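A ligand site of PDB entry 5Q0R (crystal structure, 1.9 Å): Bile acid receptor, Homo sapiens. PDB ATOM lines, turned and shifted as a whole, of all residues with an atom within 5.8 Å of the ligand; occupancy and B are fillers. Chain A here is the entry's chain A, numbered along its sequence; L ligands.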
ATOM      1  N   PHE A  45     -15.150 -20.351 -19.902  1.00  0.00           N
ATOM      2  CA  PHE A  45     -15.889 -20.075 -18.661  1.00  0.00           C
ATOM      3  C   PHE A  45     -15.061 -20.468 -17.432  1.00  0.00           C
ATOM      4  O   PHE A  45     -15.038 -19.725 -16.448  1.00  0.00           O
ATOM      5  CB  PHE A  45     -17.245 -20.825 -18.653  1.00  0.00           C
ATOM      6  CG  PHE A  45     -18.201 -20.371 -17.565  1.00  0.00           C
ATOM      7  CD1 PHE A  45     -18.219 -21.003 -16.332  1.00  0.00           C
ATOM      8  CD2 PHE A  45     -19.075 -19.319 -17.784  1.00  0.00           C
ATOM      9  CE1 PHE A  45     -19.098 -20.584 -15.323  1.00  0.00           C
ATOM     10  CE2 PHE A  45     -19.965 -18.908 -16.781  1.00  0.00           C
ATOM     11  CZ  PHE A  45     -19.964 -19.534 -15.557  1.00  0.00           C
ATOM     12  N   LEU A  46     -14.380 -21.635 -17.490  1.00  0.00           N
ATOM     13  CA  LEU A  46     -13.535 -22.124 -16.417  1.00  0.00           C
ATOM     14  C   LEU A  46     -12.326 -21.223 -16.176  1.00  0.00           C
ATOM     15  O   LEU A  46     -11.952 -21.014 -15.013  1.00  0.00           O
ATOM     16  CB  LEU A  46     -13.111 -23.579 -16.676  1.00  0.00           C
ATOM     17  CG  LEU A  46     -14.201 -24.633 -16.397  1.00  0.00           C
ATOM     18  CD1 LEU A  46     -13.984 -25.884 -17.226  1.00  0.00           C
ATOM     19  CD2 LEU A  46     -14.286 -24.964 -14.918  1.00  0.00           C
ATOM     20  N   LEU A  48     -12.258 -17.908 -16.665  1.00  0.00           N
ATOM     21  CA  LEU A  48     -12.810 -16.735 -15.990  1.00  0.00           C
ATOM     22  C   LEU A  48     -13.069 -17.017 -14.509  1.00  0.00           C
ATOM     23  O   LEU A  48     -12.783 -16.165 -13.661  1.00  0.00           O
ATOM     24  CB  LEU A  48     -14.062 -16.221 -16.701  1.00  0.00           C
ATOM     25  CG  LEU A  48     -13.816 -15.503 -18.039  1.00  0.00           C
ATOM     26  CD1 LEU A  48     -15.121 -15.162 -18.734  1.00  0.00           C
ATOM     27  CD2 LEU A  48     -13.002 -14.244 -17.843  1.00  0.00           C
ATOM     28  N   THR A  49     -13.549 -18.235 -14.213  1.00  0.00           N
ATOM     29  CA  THR A  49     -13.822 -18.758 -12.864  1.00  0.00           C
ATOM     30  C   THR A  49     -12.521 -18.779 -12.045  1.00  0.00           C
ATOM     31  O   THR A  49     -12.483 -18.238 -10.944  1.00  0.00           O
ATOM     32  CB  THR A  49     -14.501 -20.141 -12.994  1.00  0.00           C
ATOM     33  OG1 THR A  49     -15.699 -19.993 -13.760  1.00  0.00           O
ATOM     34  CG2 THR A  49     -14.884 -20.738 -11.675  1.00  0.00           C
ATOM     35  N   MET A  51      -9.844 -17.026 -12.663  1.00  0.00           N
ATOM     36  CA  MET A  51      -9.424 -15.622 -12.520  1.00  0.00           C
ATOM     37  C   MET A  51     -10.190 -14.908 -11.398  1.00  0.00           C
ATOM     38  O   MET A  51      -9.580 -14.197 -10.597  1.00  0.00           O
ATOM     39  CB  MET A  51      -9.540 -14.856 -13.854  1.00  0.00           C
ATOM     40  CG  MET A  51      -8.518 -15.302 -14.886  1.00  0.00           C
ATOM     41  SD  MET A  51      -8.629 -14.451 -16.496  1.00  0.00           S
ATOM     42  CE  MET A  51      -7.741 -12.926 -16.097  1.00  0.00           C
ATOM     43  N   ALA A  52     -11.507 -15.092 -11.338  1.00  0.00           N
ATOM     44  CA  ALA A  52     -12.338 -14.475 -10.311  1.00  0.00           C
ATOM     45  C   ALA A  52     -12.023 -15.035  -8.910  1.00  0.00           C
ATOM     46  O   ALA A  52     -12.055 -14.275  -7.946  1.00  0.00           O
ATOM     47  CB  ALA A  52     -13.819 -14.640 -10.650  1.00  0.00           C
ATOM     48  N   HIS A  55      -8.709 -13.507  -7.783  1.00  0.00           N
ATOM     49  CA  HIS A  55      -8.964 -12.135  -7.378  1.00  0.00           C
ATOM     50  C   HIS A  55      -9.576 -12.006  -5.966  1.00  0.00           C
ATOM     51  O   HIS A  55      -9.146 -11.118  -5.224  1.00  0.00           O
ATOM     52  CB  HIS A  55      -9.808 -11.376  -8.403  1.00  0.00           C
ATOM     53  CG  HIS A  55     -10.099  -9.971  -7.983  1.00  0.00           C
ATOM     54  ND1 HIS A  55     -11.331  -9.622  -7.466  1.00  0.00           N
ATOM     55  CD2 HIS A  55      -9.258  -8.922  -7.874  1.00  0.00           C
ATOM     56  CE1 HIS A  55     -11.220  -8.359  -7.108  1.00  0.00           C
ATOM     57  NE2 HIS A  55      -9.998  -7.887  -7.344  1.00  0.00           N
ATOM     58  N   MET A  89     -13.787  -6.480  -8.480  1.00  0.00           N
ATOM     59  CA  MET A  89     -13.483  -7.376  -9.600  1.00  0.00           C
ATOM     60  C   MET A  89     -13.494  -6.609 -10.929  1.00  0.00           C
ATOM     61  O   MET A  89     -12.528  -6.702 -11.690  1.00  0.00           O
ATOM     62  CB  MET A  89     -14.469  -8.547  -9.618  1.00  0.00           C
ATOM     63  CG  MET A  89     -14.397  -9.383 -10.875  1.00  0.00           C
ATOM     64  SD  MET A  89     -15.388 -10.868 -10.757  1.00  0.00           S
ATOM     65  CE  MET A  89     -17.063 -10.160 -10.798  1.00  0.00           C
ATOM     66  N   PHE A  90     -14.578  -5.863 -11.213  1.00  0.00           N
ATOM     67  CA  PHE A  90     -14.695  -5.078 -12.437  1.00  0.00           C
ATOM     68  C   PHE A  90     -13.646  -3.980 -12.532  1.00  0.00           C
ATOM     69  O   PHE A  90     -13.149  -3.710 -13.627  1.00  0.00           O
ATOM     70  CB  PHE A  90     -16.103  -4.495 -12.598  1.00  0.00           C
ATOM     71  CG  PHE A  90     -17.073  -5.472 -13.194  1.00  0.00           C
ATOM     72  CD1 PHE A  90     -17.091  -5.728 -14.559  1.00  0.00           C
ATOM     73  CD2 PHE A  90     -17.988  -6.141 -12.381  1.00  0.00           C
ATOM     74  CE1 PHE A  90     -17.979  -6.657 -15.110  1.00  0.00           C
ATOM     75  CE2 PHE A  90     -18.902  -7.047 -12.944  1.00  0.00           C
ATOM     76  CZ  PHE A  90     -18.882  -7.304 -14.293  1.00  0.00           C
ATOM     77  N   ARG A  92     -10.570  -4.076 -11.076  1.00  0.00           N
ATOM     78  CA  ARG A  92      -9.313  -4.778 -11.335  1.00  0.00           C
ATOM     79  C   ARG A  92      -9.257  -5.271 -12.797  1.00  0.00           C
ATOM     80  O   ARG A  92      -8.209  -5.170 -13.434  1.00  0.00           O
ATOM     81  CB  ARG A  92      -9.105  -5.911 -10.309  1.00  0.00           C
ATOM     82  CG  ARG A  92      -7.824  -6.725 -10.472  1.00  0.00           C
ATOM     83  CD  ARG A  92      -6.539  -5.932 -10.459  1.00  0.00           C
ATOM     84  NE  ARG A  92      -5.422  -6.846 -10.658  1.00  0.00           N
ATOM     85  CZ  ARG A  92      -4.209  -6.492 -11.081  1.00  0.00           C
ATOM     86  NH1 ARG A  92      -3.940  -5.230 -11.367  1.00  0.00           N
ATOM     87  NH2 ARG A  92      -3.265  -7.410 -11.229  1.00  0.00           N
ATOM     88  N   SER A  93     -10.393  -5.792 -13.312  1.00  0.00           N
ATOM     89  CA  SER A  93     -10.451  -6.268 -14.687  1.00  0.00           C
ATOM     90  C   SER A  93     -10.252  -5.118 -15.688  1.00  0.00           C
ATOM     91  O   SER A  93      -9.591  -5.310 -16.718  1.00  0.00           O
ATOM     92  CB  SER A  93     -11.734  -7.065 -14.944  1.00  0.00           C
ATOM     93  OG  SER A  93     -12.900  -6.254 -15.004  1.00  0.00           O
ATOM     94  N   ALA A  94     -10.725  -3.902 -15.355  1.00  0.00           N
ATOM     95  CA  ALA A  94     -10.525  -2.713 -16.182  1.00  0.00           C
ATOM     96  C   ALA A  94      -9.046  -2.333 -16.235  1.00  0.00           C
ATOM     97  O   ALA A  94      -8.538  -1.997 -17.306  1.00  0.00           O
ATOM     98  CB  ALA A  94     -11.356  -1.551 -15.661  1.00  0.00           C
ATOM     99  N   ILE A  96      -6.274  -4.348 -15.754  1.00  0.00           N
ATOM    100  CA  ILE A  96      -5.596  -5.403 -16.509  1.00  0.00           C
ATOM    101  C   ILE A  96      -5.785  -5.178 -18.025  1.00  0.00           C
ATOM    102  O   ILE A  96      -4.843  -5.321 -18.806  1.00  0.00           O
ATOM    103  CB  ILE A  96      -6.133  -6.805 -16.039  1.00  0.00           C
ATOM    104  CG1 ILE A  96      -5.532  -7.212 -14.687  1.00  0.00           C
ATOM    105  CG2 ILE A  96      -5.940  -7.906 -17.090  1.00  0.00           C
ATOM    106  CD1 ILE A  96      -6.306  -8.355 -13.953  1.00  0.00           C
ATOM    107  N   PHE A  97      -7.020  -4.846 -18.419  1.00  0.00           N
ATOM    108  CA  PHE A  97      -7.381  -4.627 -19.830  1.00  0.00           C
ATOM    109  C   PHE A  97      -6.606  -3.439 -20.411  1.00  0.00           C
ATOM    110  O   PHE A  97      -6.077  -3.542 -21.507  1.00  0.00           O
ATOM    111  CB  PHE A  97      -8.909  -4.442 -19.993  1.00  0.00           C
ATOM    112  CG  PHE A  97      -9.369  -4.057 -21.390  1.00  0.00           C
ATOM    113  CD1 PHE A  97      -9.676  -5.039 -22.330  1.00  0.00           C
ATOM    114  CD2 PHE A  97      -9.524  -2.721 -21.743  1.00  0.00           C
ATOM    115  CE1 PHE A  97     -10.103  -4.673 -23.619  1.00  0.00           C
ATOM    116  CE2 PHE A  97      -9.956  -2.370 -23.039  1.00  0.00           C
ATOM    117  CZ  PHE A  97     -10.243  -3.344 -23.956  1.00  0.00           C
ATOM    118  N   LEU A 101      -1.825  -7.215 -19.165  1.00  0.00           N
ATOM    119  CA  LEU A 101      -1.729  -8.236 -20.208  1.00  0.00           C
ATOM    120  C   LEU A 101      -1.170  -7.742 -21.561  1.00  0.00           C
ATOM    121  O   LEU A 101      -1.581  -6.687 -22.048  1.00  0.00           O
ATOM    122  CB  LEU A 101      -3.072  -8.967 -20.409  1.00  0.00           C
ATOM    123  CG  LEU A 101      -3.237 -10.261 -19.614  1.00  0.00           C
ATOM    124  CD1 LEU A 101      -4.670 -10.526 -19.313  1.00  0.00           C
ATOM    125  CD2 LEU A 101      -2.655 -11.466 -20.367  1.00  0.00           C
ATOM    126  N   SER A 106      -3.779 -10.321 -24.480  1.00  0.00           N
ATOM    127  CA  SER A 106      -5.051  -9.686 -24.120  1.00  0.00           C
ATOM    128  C   SER A 106      -6.075  -9.914 -25.222  1.00  0.00           C
ATOM    129  O   SER A 106      -7.261 -10.068 -24.926  1.00  0.00           O
ATOM    130  CB  SER A 106      -4.883  -8.201 -23.849  1.00  0.00           C
ATOM    131  OG  SER A 106      -4.375  -7.501 -24.980  1.00  0.00           O
ATOM    132  N   ASP A 107      -5.619  -9.981 -26.496  1.00  0.00           N
ATOM    133  CA  ASP A 107      -6.499 -10.258 -27.631  1.00  0.00           C
ATOM    134  C   ASP A 107      -7.090 -11.663 -27.502  1.00  0.00           C
ATOM    135  O   ASP A 107      -8.261 -11.861 -27.811  1.00  0.00           O
ATOM    136  CB  ASP A 107      -5.754 -10.089 -28.973  1.00  0.00           C
ATOM    137  CG  ASP A 107      -5.533  -8.653 -29.404  1.00  0.00           C
ATOM    138  OD1 ASP A 107      -6.277  -7.759 -28.928  1.00  0.00           O
ATOM    139  OD2 ASP A 107      -4.635  -8.414 -30.245  1.00  0.00           O
ATOM    140  N   LEU A 109      -7.465 -13.333 -24.519  1.00  0.00           N
ATOM    141  CA  LEU A 109      -8.387 -13.304 -23.385  1.00  0.00           C
ATOM    142  C   LEU A 109      -9.736 -12.663 -23.767  1.00  0.00           C
ATOM    143  O   LEU A 109     -10.783 -13.181 -23.369  1.00  0.00           O
ATOM    144  CB  LEU A 109      -7.785 -12.625 -22.143  1.00  0.00           C
ATOM    145  CG  LEU A 109      -8.695 -12.557 -20.895  1.00  0.00           C
ATOM    146  CD1 LEU A 109      -9.154 -13.936 -20.430  1.00  0.00           C
ATOM    147  CD2 LEU A 109      -8.034 -11.837 -19.773  1.00  0.00           C
ATOM    148  N   GLU A 110      -9.696 -11.575 -24.576  1.00  0.00           N
ATOM    149  CA  GLU A 110     -10.901 -10.921 -25.074  1.00  0.00           C
ATOM    150  C   GLU A 110     -11.726 -11.912 -25.907  1.00  0.00           C
ATOM    151  O   GLU A 110     -12.935 -12.032 -25.703  1.00  0.00           O
ATOM    152  CB  GLU A 110     -10.554  -9.654 -25.877  1.00  0.00           C
ATOM    153  CG  GLU A 110     -11.755  -8.937 -26.448  1.00  0.00           C
ATOM    154  CD  GLU A 110     -11.582  -7.474 -26.790  1.00  0.00           C
ATOM    155  OE1 GLU A 110     -10.503  -6.902 -26.507  1.00  0.00           O
ATOM    156  OE2 GLU A 110     -12.557  -6.883 -27.318  1.00  0.00           O
ATOM    157  N   ILE A 113     -13.439 -14.289 -23.451  1.00  0.00           N
ATOM    158  CA  ILE A 113     -14.560 -13.623 -22.766  1.00  0.00           C
ATOM    159  C   ILE A 113     -15.774 -13.519 -23.688  1.00  0.00           C
ATOM    160  O   ILE A 113     -16.890 -13.815 -23.260  1.00  0.00           O
ATOM    161  CB  ILE A 113     -14.124 -12.257 -22.150  1.00  0.00           C
ATOM    162  CG1 ILE A 113     -13.256 -12.486 -20.895  1.00  0.00           C
ATOM    163  CG2 ILE A 113     -15.349 -11.363 -21.808  1.00  0.00           C
ATOM    164  CD1 ILE A 113     -12.406 -11.359 -20.507  1.00  0.00           C
ATOM    165  N   SER A 116     -17.607 -17.235 -23.941  1.00  0.00           N
ATOM    166  CA  SER A 116     -17.662 -17.914 -22.642  1.00  0.00           C
ATOM    167  C   SER A 116     -19.098 -18.218 -22.170  1.00  0.00           C
ATOM    168  O   SER A 116     -19.287 -18.737 -21.062  1.00  0.00           O
ATOM    169  CB  SER A 116     -16.945 -17.084 -21.578  1.00  0.00           C
ATOM    170  OG  SER A 116     -17.621 -15.851 -21.427  1.00  0.00           O
ATOM    171  N   ILE A 118     -21.390 -15.810 -21.842  1.00  0.00           N
ATOM    172  CA  ILE A 118     -21.894 -14.564 -21.252  1.00  0.00           C
ATOM    173  C   ILE A 118     -22.686 -13.846 -22.355  1.00  0.00           C
ATOM    174  O   ILE A 118     -22.181 -13.693 -23.468  1.00  0.00           O
ATOM    175  CB  ILE A 118     -20.754 -13.648 -20.711  1.00  0.00           C
ATOM    176  CG1 ILE A 118     -19.943 -14.312 -19.565  1.00  0.00           C
ATOM    177  CG2 ILE A 118     -21.274 -12.261 -20.289  1.00  0.00           C
ATOM    178  CD1 ILE A 118     -18.563 -13.604 -19.281  1.00  0.00           C
ATOM    179  N   MET A 126     -19.615  -3.841 -20.016  1.00  0.00           N
ATOM    180  CA  MET A 126     -18.326  -4.245 -19.454  1.00  0.00           C
ATOM    181  C   MET A 126     -17.168  -3.651 -20.269  1.00  0.00           C
ATOM    182  O   MET A 126     -16.337  -2.937 -19.697  1.00  0.00           O
ATOM    183  CB  MET A 126     -18.242  -5.781 -19.431  1.00  0.00           C
ATOM    184  CG  MET A 126     -17.031  -6.332 -18.699  1.00  0.00           C
ATOM    185  SD  MET A 126     -16.551  -8.007 -19.247  1.00  0.00           S
ATOM    186  CE  MET A 126     -18.112  -8.896 -19.074  1.00  0.00           C
ATOM    187  N   PHE A 127     -17.112  -3.915 -21.591  1.00  0.00           N
ATOM    188  CA  PHE A 127     -16.059  -3.383 -22.461  1.00  0.00           C
ATOM    189  C   PHE A 127     -16.153  -1.862 -22.634  1.00  0.00           C
ATOM    190  O   PHE A 127     -15.120  -1.214 -22.813  1.00  0.00           O
ATOM    191  CB  PHE A 127     -15.961  -4.123 -23.804  1.00  0.00           C
ATOM    192  CG  PHE A 127     -15.211  -5.438 -23.662  1.00  0.00           C
ATOM    193  CD1 PHE A 127     -15.884  -6.634 -23.497  1.00  0.00           C
ATOM    194  CD2 PHE A 127     -13.819  -5.468 -23.677  1.00  0.00           C
ATOM    195  CE1 PHE A 127     -15.191  -7.843 -23.336  1.00  0.00           C
ATOM    196  CE2 PHE A 127     -13.120  -6.662 -23.509  1.00  0.00           C
ATOM    197  CZ  PHE A 127     -13.817  -7.850 -23.344  1.00  0.00           C
ATOM    198  N   TYR A 130     -14.465  -0.556 -19.569  1.00  0.00           N
ATOM    199  CA  TYR A 130     -13.008  -0.702 -19.764  1.00  0.00           C
ATOM    200  C   TYR A 130     -12.443   0.470 -20.565  1.00  0.00           C
ATOM    201  O   TYR A 130     -11.410   1.020 -20.191  1.00  0.00           O
ATOM    202  CB  TYR A 130     -12.674  -2.027 -20.478  1.00  0.00           C
ATOM    203  CG  TYR A 130     -12.901  -3.312 -19.698  1.00  0.00           C
ATOM    204  CD1 TYR A 130     -13.240  -3.272 -18.335  1.00  0.00           C
ATOM    205  CD2 TYR A 130     -12.791  -4.553 -20.310  1.00  0.00           C
ATOM    206  CE1 TYR A 130     -13.472  -4.450 -17.627  1.00  0.00           C
ATOM    207  CE2 TYR A 130     -13.016  -5.725 -19.606  1.00  0.00           C
ATOM    208  CZ  TYR A 130     -13.350  -5.674 -18.268  1.00  0.00           C
ATOM    209  OH  TYR A 130     -13.588  -6.833 -17.592  1.00  0.00           O
ATOM    210  N   HIS A 208     -24.264  -7.961 -12.820  1.00  0.00           N
ATOM    211  CA  HIS A 208     -23.715  -9.241 -12.350  1.00  0.00           C
ATOM    212  C   HIS A 208     -24.779 -10.152 -11.704  1.00  0.00           C
ATOM    213  O   HIS A 208     -24.794 -11.350 -11.991  1.00  0.00           O
ATOM    214  CB  HIS A 208     -22.545  -9.008 -11.374  1.00  0.00           C
ATOM    215  CG  HIS A 208     -21.772 -10.247 -11.038  1.00  0.00           C
ATOM    216  ND1 HIS A 208     -20.759 -10.712 -11.852  1.00  0.00           N
ATOM    217  CD2 HIS A 208     -21.890 -11.074  -9.965  1.00  0.00           C
ATOM    218  CE1 HIS A 208     -20.303 -11.802 -11.262  1.00  0.00           C
ATOM    219  NE2 HIS A 208     -20.953 -12.056 -10.127  1.00  0.00           N
ATOM    220  N   MET A 211     -26.884 -11.589 -14.335  1.00  0.00           N
ATOM    221  CA  MET A 211     -26.047 -12.546 -15.063  1.00  0.00           C
ATOM    222  C   MET A 211     -26.033 -13.907 -14.372  1.00  0.00           C
ATOM    223  O   MET A 211     -26.182 -14.937 -15.051  1.00  0.00           O
ATOM    224  CB  MET A 211     -24.627 -11.973 -15.223  1.00  0.00           C
ATOM    225  CG  MET A 211     -23.732 -12.767 -16.135  1.00  0.00           C
ATOM    226  SD  MET A 211     -22.273 -11.843 -16.651  1.00  0.00           S
ATOM    227  CE  MET A 211     -21.315 -11.837 -15.134  1.00  0.00           C
ATOM    228  N   TRP A 215     -28.331 -18.560 -14.980  1.00  0.00           N
ATOM    229  CA  TRP A 215     -27.918 -19.959 -14.847  1.00  0.00           C
ATOM    230  C   TRP A 215     -28.401 -20.577 -13.535  1.00  0.00           C
ATOM    231  O   TRP A 215     -29.356 -21.344 -13.541  1.00  0.00           O
ATOM    232  CB  TRP A 215     -26.384 -20.082 -14.969  1.00  0.00           C
ATOM    233  CG  TRP A 215     -25.813 -19.433 -16.205  1.00  0.00           C
ATOM    234  CD1 TRP A 215     -26.059 -19.765 -17.498  1.00  0.00           C
ATOM    235  CD2 TRP A 215     -24.882 -18.341 -16.232  1.00  0.00           C
ATOM    236  NE1 TRP A 215     -25.348 -18.957 -18.345  1.00  0.00           N
ATOM    237  CE2 TRP A 215     -24.608 -18.069 -17.597  1.00  0.00           C
ATOM    238  CE3 TRP A 215     -24.242 -17.570 -15.249  1.00  0.00           C
ATOM    239  CZ2 TRP A 215     -23.735 -17.054 -17.991  1.00  0.00           C
ATOM    240  CZ3 TRP A 215     -23.369 -16.569 -15.642  1.00  0.00           C
ATOM    241  CH2 TRP A 215     -23.127 -16.323 -17.001  1.00  0.00           C
ATOM    242  N   LEU A 226     -16.864 -17.702  -4.974  1.00  0.00           N
ATOM    243  CA  LEU A 226     -17.758 -17.045  -5.912  1.00  0.00           C
ATOM    244  C   LEU A 226     -19.203 -16.945  -5.398  1.00  0.00           C
ATOM    245  O   LEU A 226     -19.499 -15.919  -4.792  1.00  0.00           O
ATOM    246  CB  LEU A 226     -17.669 -17.643  -7.327  1.00  0.00           C
ATOM    247  CG  LEU A 226     -16.289 -17.558  -8.024  1.00  0.00           C
ATOM    248  CD1 LEU A 226     -16.394 -17.890  -9.486  1.00  0.00           C
ATOM    249  CD2 LEU A 226     -15.614 -16.216  -7.811  1.00  0.00           C
ATOM    250  N   TRP A 230     -20.809 -13.717  -3.656  1.00  0.00           N
ATOM    251  CA  TRP A 230     -21.767 -13.196  -4.643  1.00  0.00           C
ATOM    252  C   TRP A 230     -23.245 -13.414  -4.267  1.00  0.00           C
ATOM    253  O   TRP A 230     -24.104 -12.837  -4.928  1.00  0.00           O
ATOM    254  CB  TRP A 230     -21.503 -13.802  -6.019  1.00  0.00           C
ATOM    255  CG  TRP A 230     -20.208 -13.422  -6.673  1.00  0.00           C
ATOM    256  CD1 TRP A 230     -19.356 -12.417  -6.299  1.00  0.00           C
ATOM    257  CD2 TRP A 230     -19.674 -13.992  -7.871  1.00  0.00           C
ATOM    258  NE1 TRP A 230     -18.302 -12.343  -7.182  1.00  0.00           N
ATOM    259  CE2 TRP A 230     -18.476 -13.289  -8.167  1.00  0.00           C
ATOM    260  CE3 TRP A 230     -20.086 -15.015  -8.724  1.00  0.00           C
ATOM    261  CZ2 TRP A 230     -17.696 -13.598  -9.280  1.00  0.00           C
ATOM    262  CZ3 TRP A 230     -19.308 -15.329  -9.825  1.00  0.00           C
ATOM    263  CH2 TRP A 230     -18.132 -14.622 -10.099  1.00  0.00           C
HETATM  264  C1  LIG L   1     -12.522 -10.377 -16.879  1.00  0.00           C
HETATM  265  C2  LIG L   1     -17.196 -14.735 -14.196  1.00  0.00           C
HETATM  266  C3  LIG L   1     -14.734 -10.626 -16.480  1.00  0.00           C
HETATM  267  C4  LIG L   1     -13.839  -9.961 -17.205  1.00  0.00           C
HETATM  268  C5  LIG L   1     -11.209  -9.939 -17.378  1.00  0.00           C
HETATM  269  C6  LIG L   1     -11.644 -12.134 -15.165  1.00  0.00           C
HETATM  270  C7  LIG L   1     -16.791 -11.859 -15.920  1.00  0.00           C
HETATM  271  C8  LIG L   1     -16.235 -10.552 -16.460  1.00  0.00           C
HETATM  272  C9  LIG L   1     -16.632 -15.757 -13.429  1.00  0.00           C
HETATM  273  C10 LIG L   1     -11.133 -11.388 -13.951  1.00  0.00           C
HETATM  274  C11 LIG L   1     -17.856 -16.347 -15.867  1.00  0.00           C
HETATM  275  C12 LIG L   1     -11.690 -11.608 -12.697  1.00  0.00           C
HETATM  276  C13 LIG L   1      -8.233  -8.228 -20.154  1.00  0.00           C
HETATM  277  F1  LIG L   1     -18.348 -14.075 -16.157  1.00  0.00           F
HETATM  278  C14 LIG L   1     -17.796 -15.062 -15.408  1.00  0.00           C
HETATM  279  C15 LIG L   1     -17.298 -17.361 -15.097  1.00  0.00           C
HETATM  280  C16 LIG L   1     -16.687 -17.063 -13.889  1.00  0.00           C
HETATM  281  S1  LIG L   1     -17.093 -13.072 -13.562  1.00  0.00           S
HETATM  282  O1  LIG L   1     -16.383 -13.143 -12.331  1.00  0.00           O
HETATM  283  O2  LIG L   1     -18.416 -12.531 -13.583  1.00  0.00           O
HETATM  284  N1  LIG L   1     -16.187 -12.169 -14.587  1.00  0.00           N
HETATM  285  O3  LIG L   1     -10.237 -10.681 -17.396  1.00  0.00           O
HETATM  286  N2  LIG L   1     -11.161  -8.662 -17.803  1.00  0.00           N
HETATM  287  C17 LIG L   1      -9.951  -8.034 -18.334  1.00  0.00           C
HETATM  288  C18 LIG L   1      -9.569  -8.277 -19.771  1.00  0.00           C
HETATM  289  C19 LIG L   1     -10.523  -8.540 -20.749  1.00  0.00           C
HETATM  290  C20 LIG L   1     -10.154  -8.748 -22.071  1.00  0.00           C
HETATM  291  C21 LIG L   1      -8.820  -8.704 -22.441  1.00  0.00           C
HETATM  292  C22 LIG L   1      -7.858  -8.444 -21.479  1.00  0.00           C
HETATM  293  N3  LIG L   1     -12.651 -11.355 -15.890  1.00  0.00           N
HETATM  294  C23 LIG L   1     -10.101 -10.462 -14.071  1.00  0.00           C
HETATM  295  C24 LIG L   1      -9.634  -9.780 -12.965  1.00  0.00           C
HETATM  296  C25 LIG L   1     -10.195 -10.001 -11.720  1.00  0.00           C
HETATM  297  C26 LIG L   1     -11.229 -10.918 -11.588  1.00  0.00           C
HETATM  298  C27 LIG L   1     -14.076 -11.511 -15.634  1.00  0.00           C
HETATM  299  C28 LIG L   1     -14.729 -12.452 -14.662  1.00  0.00           C
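SD of Met 89 lies close to O1 of the ligand (2.9 Å).
Residues that only touch the ligand: Phe 45 (3.4 Å), Leu 48 (3.5 Å), Thr 49 (3.1 Å), Met 51 (3.6 Å), Ala 52 (3.4 Å), His 55 (3.5 Å), Ser 93 (3.2 Å), Ile 96 (3.8 Å), Phe 97 (3.7 Å), Ser 106 (3.2 Å), Leu 109 (3.4 Å), Glu 110 (3.7 Å), Ile 113 (3.4 Å), Ile 118 (3.2 Å), Met 126 (3.6 Å), Phe 127 (3.9 Å), Met 211 (3.4 Å) and Trp 230 (3.2 Å).
Within 4 Å of the ligand: Phe 45, Leu 48, Thr 49, Met 51, Ala 52, His 55, Met 89, Ser 93, Ile 96, Phe 97, Ser 106, Leu 109, Glu 110, Ile 113, Ile 118, Met 126, Phe 127, Tyr 130, His 208, Met 211 and Trp 230.
OH of Tyr 130 lies within hydrogen-bond range of N2 of the ligand (3.0 Å).
ND1 of His 208 lies close to O2 of the ligand (3.4 Å).
O of Met 89 sits at hydrogen-bond distance from OG of Ser 93 (3.4 Å).
The side-chain hydroxyl (OH) of Tyr 130 is in hydrogen-bond range of the side-chain hydroxyl (OG) of Ser 93, 2.7 Å away.
OH of Tyr 130 sits at hydrogen-bond distance from SD of Met 126 (3.6 Å).
O of Phe 45 lies within hydrogen-bond range of OG1 of Thr 49.
O of Phe 90 sits at hydrogen-bond distance from OG of Ser 93, 2.9 Å away.
The side-chain hydroxyl (OG) of Ser 116 is in hydrogen-bond range of the backbone carbonyl oxygen (O) of Ile 113, 2.8 Å away.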
